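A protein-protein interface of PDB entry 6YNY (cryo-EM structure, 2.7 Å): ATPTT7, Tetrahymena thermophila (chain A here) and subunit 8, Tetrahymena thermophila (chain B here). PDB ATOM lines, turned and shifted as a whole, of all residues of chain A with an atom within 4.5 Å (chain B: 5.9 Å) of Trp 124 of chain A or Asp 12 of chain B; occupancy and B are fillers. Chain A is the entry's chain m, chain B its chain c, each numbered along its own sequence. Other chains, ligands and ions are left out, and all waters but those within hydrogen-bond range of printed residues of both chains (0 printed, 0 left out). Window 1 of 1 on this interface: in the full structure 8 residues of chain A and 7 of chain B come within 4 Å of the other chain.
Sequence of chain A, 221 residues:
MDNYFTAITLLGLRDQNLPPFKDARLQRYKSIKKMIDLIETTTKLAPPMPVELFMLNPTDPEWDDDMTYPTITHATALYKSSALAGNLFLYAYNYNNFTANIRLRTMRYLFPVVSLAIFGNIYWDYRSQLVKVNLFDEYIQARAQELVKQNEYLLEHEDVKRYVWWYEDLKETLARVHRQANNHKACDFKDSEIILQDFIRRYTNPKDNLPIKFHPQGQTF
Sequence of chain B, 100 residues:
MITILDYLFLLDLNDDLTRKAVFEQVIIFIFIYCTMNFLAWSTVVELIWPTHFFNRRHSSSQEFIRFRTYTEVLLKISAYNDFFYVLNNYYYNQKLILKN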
ATOM      1  N   GLY A 120     -13.057  20.720   5.983  1.00  0.00           N
ATOM      2  CA  GLY A 120     -13.007  20.411   4.567  1.00  0.00           C
ATOM      3  C   GLY A 120     -11.617  20.037   4.101  1.00  0.00           C
ATOM      4  O   GLY A 120     -11.444  19.100   3.320  1.00  0.00           O
ATOM      5  N   ASN A 121     -10.605  20.761   4.573  1.00  0.00           N
ATOM      6  CA  ASN A 121      -9.235  20.433   4.210  1.00  0.00           C
ATOM      7  C   ASN A 121      -8.835  19.071   4.757  1.00  0.00           C
ATOM      8  O   ASN A 121      -8.168  18.290   4.070  1.00  0.00           O
ATOM      9  CB  ASN A 121      -8.289  21.518   4.717  1.00  0.00           C
ATOM     10  CG  ASN A 121      -6.845  21.080   4.704  1.00  0.00           C
ATOM     11  OD1 ASN A 121      -6.231  20.892   5.752  1.00  0.00           O
ATOM     12  ND2 ASN A 121      -6.299  20.897   3.515  1.00  0.00           N
ATOM     13  N   ILE A 122      -9.239  18.767   5.989  1.00  0.00           N
ATOM     14  CA  ILE A 122      -8.888  17.489   6.596  1.00  0.00           C
ATOM     15  C   ILE A 122      -9.517  16.342   5.818  1.00  0.00           C
ATOM     16  O   ILE A 122      -8.847  15.363   5.471  1.00  0.00           O
ATOM     17  CB  ILE A 122      -9.311  17.465   8.075  1.00  0.00           C
ATOM     18  CG1 ILE A 122      -8.553  18.532   8.858  1.00  0.00           C
ATOM     19  CG2 ILE A 122      -9.066  16.098   8.674  1.00  0.00           C
ATOM     20  CD1 ILE A 122      -9.071  18.747  10.248  1.00  0.00           C
ATOM     21  N   TYR A 123     -10.815  16.445   5.533  1.00  0.00           N
ATOM     22  CA  TYR A 123     -11.504  15.363   4.843  1.00  0.00           C
ATOM     23  C   TYR A 123     -11.151  15.319   3.363  1.00  0.00           C
ATOM     24  O   TYR A 123     -11.047  14.235   2.782  1.00  0.00           O
ATOM     25  CB  TYR A 123     -13.012  15.501   5.025  1.00  0.00           C
ATOM     26  CG  TYR A 123     -13.779  14.342   4.451  1.00  0.00           C
ATOM     27  CD1 TYR A 123     -13.764  13.107   5.072  1.00  0.00           C
ATOM     28  CD2 TYR A 123     -14.512  14.479   3.289  1.00  0.00           C
ATOM     29  CE1 TYR A 123     -14.454  12.043   4.550  1.00  0.00           C
ATOM     30  CE2 TYR A 123     -15.204  13.424   2.761  1.00  0.00           C
ATOM     31  CZ  TYR A 123     -15.175  12.208   3.396  1.00  0.00           C
ATOM     32  OH  TYR A 123     -15.870  11.149   2.867  1.00  0.00           O
ATOM     33  N   TRP A 124     -10.968  16.480   2.736  1.00  0.00           N
ATOM     34  CA  TRP A 124     -10.563  16.506   1.337  1.00  0.00           C
ATOM     35  C   TRP A 124      -9.286  15.708   1.126  1.00  0.00           C
ATOM     36  O   TRP A 124      -9.203  14.868   0.224  1.00  0.00           O
ATOM     37  CB  TRP A 124     -10.376  17.950   0.875  1.00  0.00           C
ATOM     38  CG  TRP A 124      -9.899  18.071  -0.529  1.00  0.00           C
ATOM     39  CD1 TRP A 124      -8.624  17.926  -0.972  1.00  0.00           C
ATOM     40  CD2 TRP A 124     -10.691  18.369  -1.679  1.00  0.00           C
ATOM     41  NE1 TRP A 124      -8.569  18.106  -2.327  1.00  0.00           N
ATOM     42  CE2 TRP A 124      -9.828  18.382  -2.786  1.00  0.00           C
ATOM     43  CE3 TRP A 124     -12.046  18.622  -1.881  1.00  0.00           C
ATOM     44  CZ2 TRP A 124     -10.274  18.640  -4.071  1.00  0.00           C
ATOM     45  CZ3 TRP A 124     -12.485  18.876  -3.157  1.00  0.00           C
ATOM     46  CH2 TRP A 124     -11.604  18.885  -4.236  1.00  0.00           C
ATOM     47  N   ASP A 125      -8.272  15.962   1.952  1.00  0.00           N
ATOM     48  CA  ASP A 125      -7.006  15.260   1.803  1.00  0.00           C
ATOM     49  C   ASP A 125      -7.168  13.769   2.062  1.00  0.00           C
ATOM     50  O   ASP A 125      -6.650  12.941   1.307  1.00  0.00           O
ATOM     51  CB  ASP A 125      -5.964  15.867   2.738  1.00  0.00           C
ATOM     52  CG  ASP A 125      -5.635  17.303   2.389  1.00  0.00           C
ATOM     53  OD1 ASP A 125      -5.838  17.691   1.221  1.00  0.00           O
ATOM     54  OD2 ASP A 125      -5.168  18.044   3.277  1.00  0.00           O
ATOM     55  N   TYR A 126      -7.890  13.406   3.122  1.00  0.00           N
ATOM     56  CA  TYR A 126      -8.139  11.997   3.397  1.00  0.00           C
ATOM     57  C   TYR A 126      -8.918  11.345   2.264  1.00  0.00           C
ATOM     58  O   TYR A 126      -8.599  10.228   1.843  1.00  0.00           O
ATOM     59  CB  TYR A 126      -8.890  11.853   4.717  1.00  0.00           C
ATOM     60  CG  TYR A 126      -9.434  10.473   4.977  1.00  0.00           C
ATOM     61  CD1 TYR A 126      -8.643   9.489   5.540  1.00  0.00           C
ATOM     62  CD2 TYR A 126     -10.744  10.157   4.666  1.00  0.00           C
ATOM     63  CE1 TYR A 126      -9.139   8.231   5.779  1.00  0.00           C
ATOM     64  CE2 TYR A 126     -11.247   8.905   4.901  1.00  0.00           C
ATOM     65  CZ  TYR A 126     -10.441   7.943   5.458  1.00  0.00           C
ATOM     66  OH  TYR A 126     -10.941   6.685   5.697  1.00  0.00           O
ATOM     67  N   ARG A 127      -9.938  12.030   1.752  1.00  0.00           N
ATOM     68  CA  ARG A 127     -10.751  11.461   0.684  1.00  0.00           C
ATOM     69  C   ARG A 127      -9.945  11.292  -0.596  1.00  0.00           C
ATOM     70  O   ARG A 127     -10.039  10.253  -1.260  1.00  0.00           O
ATOM     71  CB  ARG A 127     -11.969  12.345   0.438  1.00  0.00           C
ATOM     72  CG  ARG A 127     -12.907  11.844  -0.633  1.00  0.00           C
ATOM     73  CD  ARG A 127     -13.608  10.579  -0.217  1.00  0.00           C
ATOM     74  NE  ARG A 127     -14.526  10.115  -1.247  1.00  0.00           N
ATOM     75  CZ  ARG A 127     -15.393   9.125  -1.081  1.00  0.00           C
ATOM     76  NH1 ARG A 127     -15.465   8.492   0.078  1.00  0.00           N
ATOM     77  NH2 ARG A 127     -16.190   8.772  -2.076  1.00  0.00           N
ATOM     78  N   SER A 128      -9.152  12.296  -0.964  1.00  0.00           N
ATOM     79  CA  SER A 128      -8.346  12.191  -2.174  1.00  0.00           C
ATOM     80  C   SER A 128      -7.309  11.083  -2.047  1.00  0.00           C
ATOM     81  O   SER A 128      -7.137  10.272  -2.961  1.00  0.00           O
ATOM     82  CB  SER A 128      -7.677  13.530  -2.473  1.00  0.00           C
ATOM     83  OG  SER A 128      -7.021  14.037  -1.332  1.00  0.00           O
ATOM     84  N   LEU B   8     -14.444  24.415  -4.363  1.00  0.00           N
ATOM     85  CA  LEU B   8     -13.995  23.643  -3.215  1.00  0.00           C
ATOM     86  C   LEU B   8     -12.605  23.061  -3.406  1.00  0.00           C
ATOM     87  O   LEU B   8     -12.045  22.520  -2.447  1.00  0.00           O
ATOM     88  CB  LEU B   8     -14.984  22.518  -2.926  1.00  0.00           C
ATOM     89  CG  LEU B   8     -16.374  22.951  -2.476  1.00  0.00           C
ATOM     90  CD1 LEU B   8     -17.256  21.744  -2.318  1.00  0.00           C
ATOM     91  CD2 LEU B   8     -16.298  23.732  -1.176  1.00  0.00           C
ATOM     92  N   PHE B   9     -12.037  23.153  -4.607  1.00  0.00           N
ATOM     93  CA  PHE B   9     -10.685  22.659  -4.822  1.00  0.00           C
ATOM     94  C   PHE B   9      -9.670  23.430  -3.995  1.00  0.00           C
ATOM     95  O   PHE B   9      -8.547  22.953  -3.803  1.00  0.00           O
ATOM     96  CB  PHE B   9     -10.314  22.742  -6.303  1.00  0.00           C
ATOM     97  CG  PHE B   9     -11.200  21.928  -7.207  1.00  0.00           C
ATOM     98  CD1 PHE B   9     -12.193  21.115  -6.695  1.00  0.00           C
ATOM     99  CD2 PHE B   9     -11.028  21.969  -8.577  1.00  0.00           C
ATOM    100  CE1 PHE B   9     -12.997  20.373  -7.528  1.00  0.00           C
ATOM    101  CE2 PHE B   9     -11.830  21.225  -9.411  1.00  0.00           C
ATOM    102  CZ  PHE B   9     -12.812  20.427  -8.884  1.00  0.00           C
ATOM    103  N   LEU B  10     -10.042  24.610  -3.501  1.00  0.00           N
ATOM    104  CA  LEU B  10      -9.164  25.396  -2.649  1.00  0.00           C
ATOM    105  C   LEU B  10      -8.852  24.703  -1.333  1.00  0.00           C
ATOM    106  O   LEU B  10      -7.921  25.121  -0.638  1.00  0.00           O
ATOM    107  CB  LEU B  10      -9.804  26.754  -2.373  1.00  0.00           C
ATOM    108  CG  LEU B  10     -10.205  27.550  -3.613  1.00  0.00           C
ATOM    109  CD1 LEU B  10     -10.857  28.854  -3.207  1.00  0.00           C
ATOM    110  CD2 LEU B  10      -9.009  27.806  -4.505  1.00  0.00           C
ATOM    111  N   LEU B  11      -9.604  23.667  -0.975  1.00  0.00           N
ATOM    112  CA  LEU B  11      -9.354  22.920   0.245  1.00  0.00           C
ATOM    113  C   LEU B  11      -8.182  21.958   0.122  1.00  0.00           C
ATOM    114  O   LEU B  11      -7.768  21.380   1.132  1.00  0.00           O
ATOM    115  CB  LEU B  11     -10.608  22.144   0.638  1.00  0.00           C
ATOM    116  CG  LEU B  11     -11.877  22.977   0.821  1.00  0.00           C
ATOM    117  CD1 LEU B  11     -13.067  22.089   1.085  1.00  0.00           C
ATOM    118  CD2 LEU B  11     -11.712  23.973   1.943  1.00  0.00           C
ATOM    119  N   ASP B  12      -7.638  21.776  -1.074  1.00  0.00           N
ATOM    120  CA  ASP B  12      -6.572  20.811  -1.287  1.00  0.00           C
ATOM    121  C   ASP B  12      -5.238  21.342  -0.784  1.00  0.00           C
ATOM    122  O   ASP B  12      -4.880  22.497  -1.019  1.00  0.00           O
ATOM    123  CB  ASP B  12      -6.456  20.461  -2.769  1.00  0.00           C
ATOM    124  CG  ASP B  12      -5.479  19.336  -3.026  1.00  0.00           C
ATOM    125  OD1 ASP B  12      -5.826  18.169  -2.757  1.00  0.00           O
ATOM    126  OD2 ASP B  12      -4.358  19.620  -3.493  1.00  0.00           O
ATOM    127  N   LEU B  13      -4.505  20.478  -0.083  1.00  0.00           N
ATOM    128  CA  LEU B  13      -3.129  20.746   0.295  1.00  0.00           C
ATOM    129  C   LEU B  13      -2.181  19.619  -0.077  1.00  0.00           C
ATOM    130  O   LEU B  13      -0.966  19.792   0.062  1.00  0.00           O
ATOM    131  CB  LEU B  13      -3.019  21.009   1.802  1.00  0.00           C
ATOM    132  CG  LEU B  13      -3.577  22.335   2.313  1.00  0.00           C
ATOM    133  CD1 LEU B  13      -3.371  22.448   3.807  1.00  0.00           C
ATOM    134  CD2 LEU B  13      -2.928  23.505   1.604  1.00  0.00           C
ATOM    135  N   ASN B  14      -2.689  18.477  -0.543  1.00  0.00           N
ATOM    136  CA  ASN B  14      -1.811  17.402  -0.981  1.00  0.00           C
ATOM    137  C   ASN B  14      -1.083  17.774  -2.263  1.00  0.00           C
ATOM    138  O   ASN B  14       0.085  17.414  -2.448  1.00  0.00           O
ATOM    139  CB  ASN B  14      -2.613  16.120  -1.197  1.00  0.00           C
ATOM    140  CG  ASN B  14      -3.237  15.598   0.069  1.00  0.00           C
ATOM    141  OD1 ASN B  14      -2.757  15.855   1.171  1.00  0.00           O
ATOM    142  ND2 ASN B  14      -4.313  14.845  -0.084  1.00  0.00           N
ATOM    143  N   ASP B  15      -1.757  18.491  -3.157  1.00  0.00           N
ATOM    144  CA  ASP B  15      -1.222  18.829  -4.468  1.00  0.00           C
ATOM    145  C   ASP B  15      -1.052  20.334  -4.635  1.00  0.00           C
ATOM    146  O   ASP B  15      -1.092  20.850  -5.752  1.00  0.00           O
ATOM    147  CB  ASP B  15      -2.125  18.271  -5.563  1.00  0.00           C
ATOM    148  CG  ASP B  15      -2.314  16.773  -5.453  1.00  0.00           C
ATOM    149  OD1 ASP B  15      -1.315  16.061  -5.222  1.00  0.00           O
ATOM    150  OD2 ASP B  15      -3.465  16.308  -5.585  1.00  0.00           O
ATOM    151  N   ASP B  16      -0.862  21.052  -3.530  1.00  0.00           N
ATOM    152  CA  ASP B  16      -0.664  22.491  -3.614  1.00  0.00           C
ATOM    153  C   ASP B  16       0.640  22.847  -4.311  1.00  0.00           C
ATOM    154  O   ASP B  16       0.759  23.953  -4.845  1.00  0.00           O
ATOM    155  CB  ASP B  16      -0.692  23.113  -2.220  1.00  0.00           C
ATOM    156  CG  ASP B  16      -0.792  24.625  -2.260  1.00  0.00           C
ATOM    157  OD1 ASP B  16      -1.145  25.170  -3.325  1.00  0.00           O
ATOM    158  OD2 ASP B  16      -0.509  25.269  -1.228  1.00  0.00           O
ATOM    159  N   ARG B  19       0.292  24.139  -8.027  1.00  0.00           N
ATOM    160  CA  ARG B  19      -0.203  25.450  -8.420  1.00  0.00           C
ATOM    161  C   ARG B  19       0.667  26.596  -7.919  1.00  0.00           C
ATOM    162  O   ARG B  19       1.201  27.356  -8.730  1.00  0.00           O
ATOM    163  CB  ARG B  19      -1.639  25.635  -7.909  1.00  0.00           C
ATOM    164  CG  ARG B  19      -2.710  24.882  -8.683  1.00  0.00           C
ATOM    165  CD  ARG B  19      -3.145  23.612  -7.997  1.00  0.00           C
ATOM    166  NE  ARG B  19      -3.584  23.838  -6.628  1.00  0.00           N
ATOM    167  CZ  ARG B  19      -4.049  22.886  -5.829  1.00  0.00           C
ATOM    168  NH1 ARG B  19      -4.151  21.638  -6.258  1.00  0.00           N
ATOM    169  NH2 ARG B  19      -4.417  23.185  -4.596  1.00  0.00           N
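The indole nitrogen of Trp 124 of chain A lies within hydrogen-bond range of the side-chain carboxylate of Asp 12 of chain B.
The side-chain hydroxyl (OG) of Ser 128 of chain A lies within hydrogen-bond range of the side-chain amide nitrogen (ND2) of Asn 14 of chain B, 3.1 Å away.
The backbone carbonyl oxygen (O) of Asp 125 of chain A sits close to the side-chain amide nitrogen (ND2) of Asn 14 of chain B, 3.3 Å away.
The side-chain carboxylate of Asp 125 of chain A lies within hydrogen-bond range of the backbone NH of Leu 13 of chain B (3.4 Å).
O of Leu 11 of chain B is in hydrogen-bond range of ND2 of Asn 121 of chain A, at 2.8 Å.
The backbone carbonyl oxygen of Asp 125 of chain A is in hydrogen-bond range of the side-chain hydroxyl of Ser 128 of chain A, 2.9 Å away.
O of Trp 124 of chain A sits at hydrogen-bond distance from OG of Ser 128 of chain A, at 2.8 Å.
ND2 of Asn 121 of chain A sits at hydrogen-bond distance from OD2 of Asp 125 of chain A, at 3.1 Å.
The side-chain carboxylate of Asp 12 of chain B is in hydrogen-bond range of the backbone NH of Asp 15 of chain B, 2.9 Å away.
OD2 of Asp 12 of chain B lies within salt-bridge range of NH1 of Arg 19 of chain B.
Among the printed residues, pairs that only touch across the chains: Gly 120 of chain A with Leu 11 of chain B (3.9 Å), Asn 121 of chain A with Leu 13 of chain B (3.3 Å), Trp 124 of chain A with Leu 8 of chain B (3.7 Å) and Trp 124 of chain A with Phe 9 of chain B (3.4 Å).
Of chain B, only Leu 8 (3.7 Å), Phe 9 (3.4 Å) and Asp 12 (2.8 Å) come within 4 Å of Trp 124 of chain A.
Of the printed residues of chain A, Asp 12 of chain B touches Trp 124 (2.8 Å).
Of the printed residues of chain B, Ser 128 of chain A touches Asn 14 (3.1 Å).
Of the printed residues of chain A, Leu 8 of chain B touches Trp 124 (3.7 Å).
Printed residues of chain A within 4 Å of Asn 14 of chain B: Asp 125 and Ser 128.
Of the 9 printed residues of chain A, 5 touch a printed residue of chain B.
Hydrophobic or aromatic side chains of chain A within 4 Å of the printed part of chain B: Trp 124.
Hydrophobic or aromatic side chains of chain B that line the printed part of chain A: Phe 9, Leu 11 and Leu 13.
Among the printed residues, 9 pairs touch across the chains.
Among the printed residues, no Asp or Glu carboxylate lies within 4 Å of a Lys or Arg side-chain nitrogen of the other chain.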
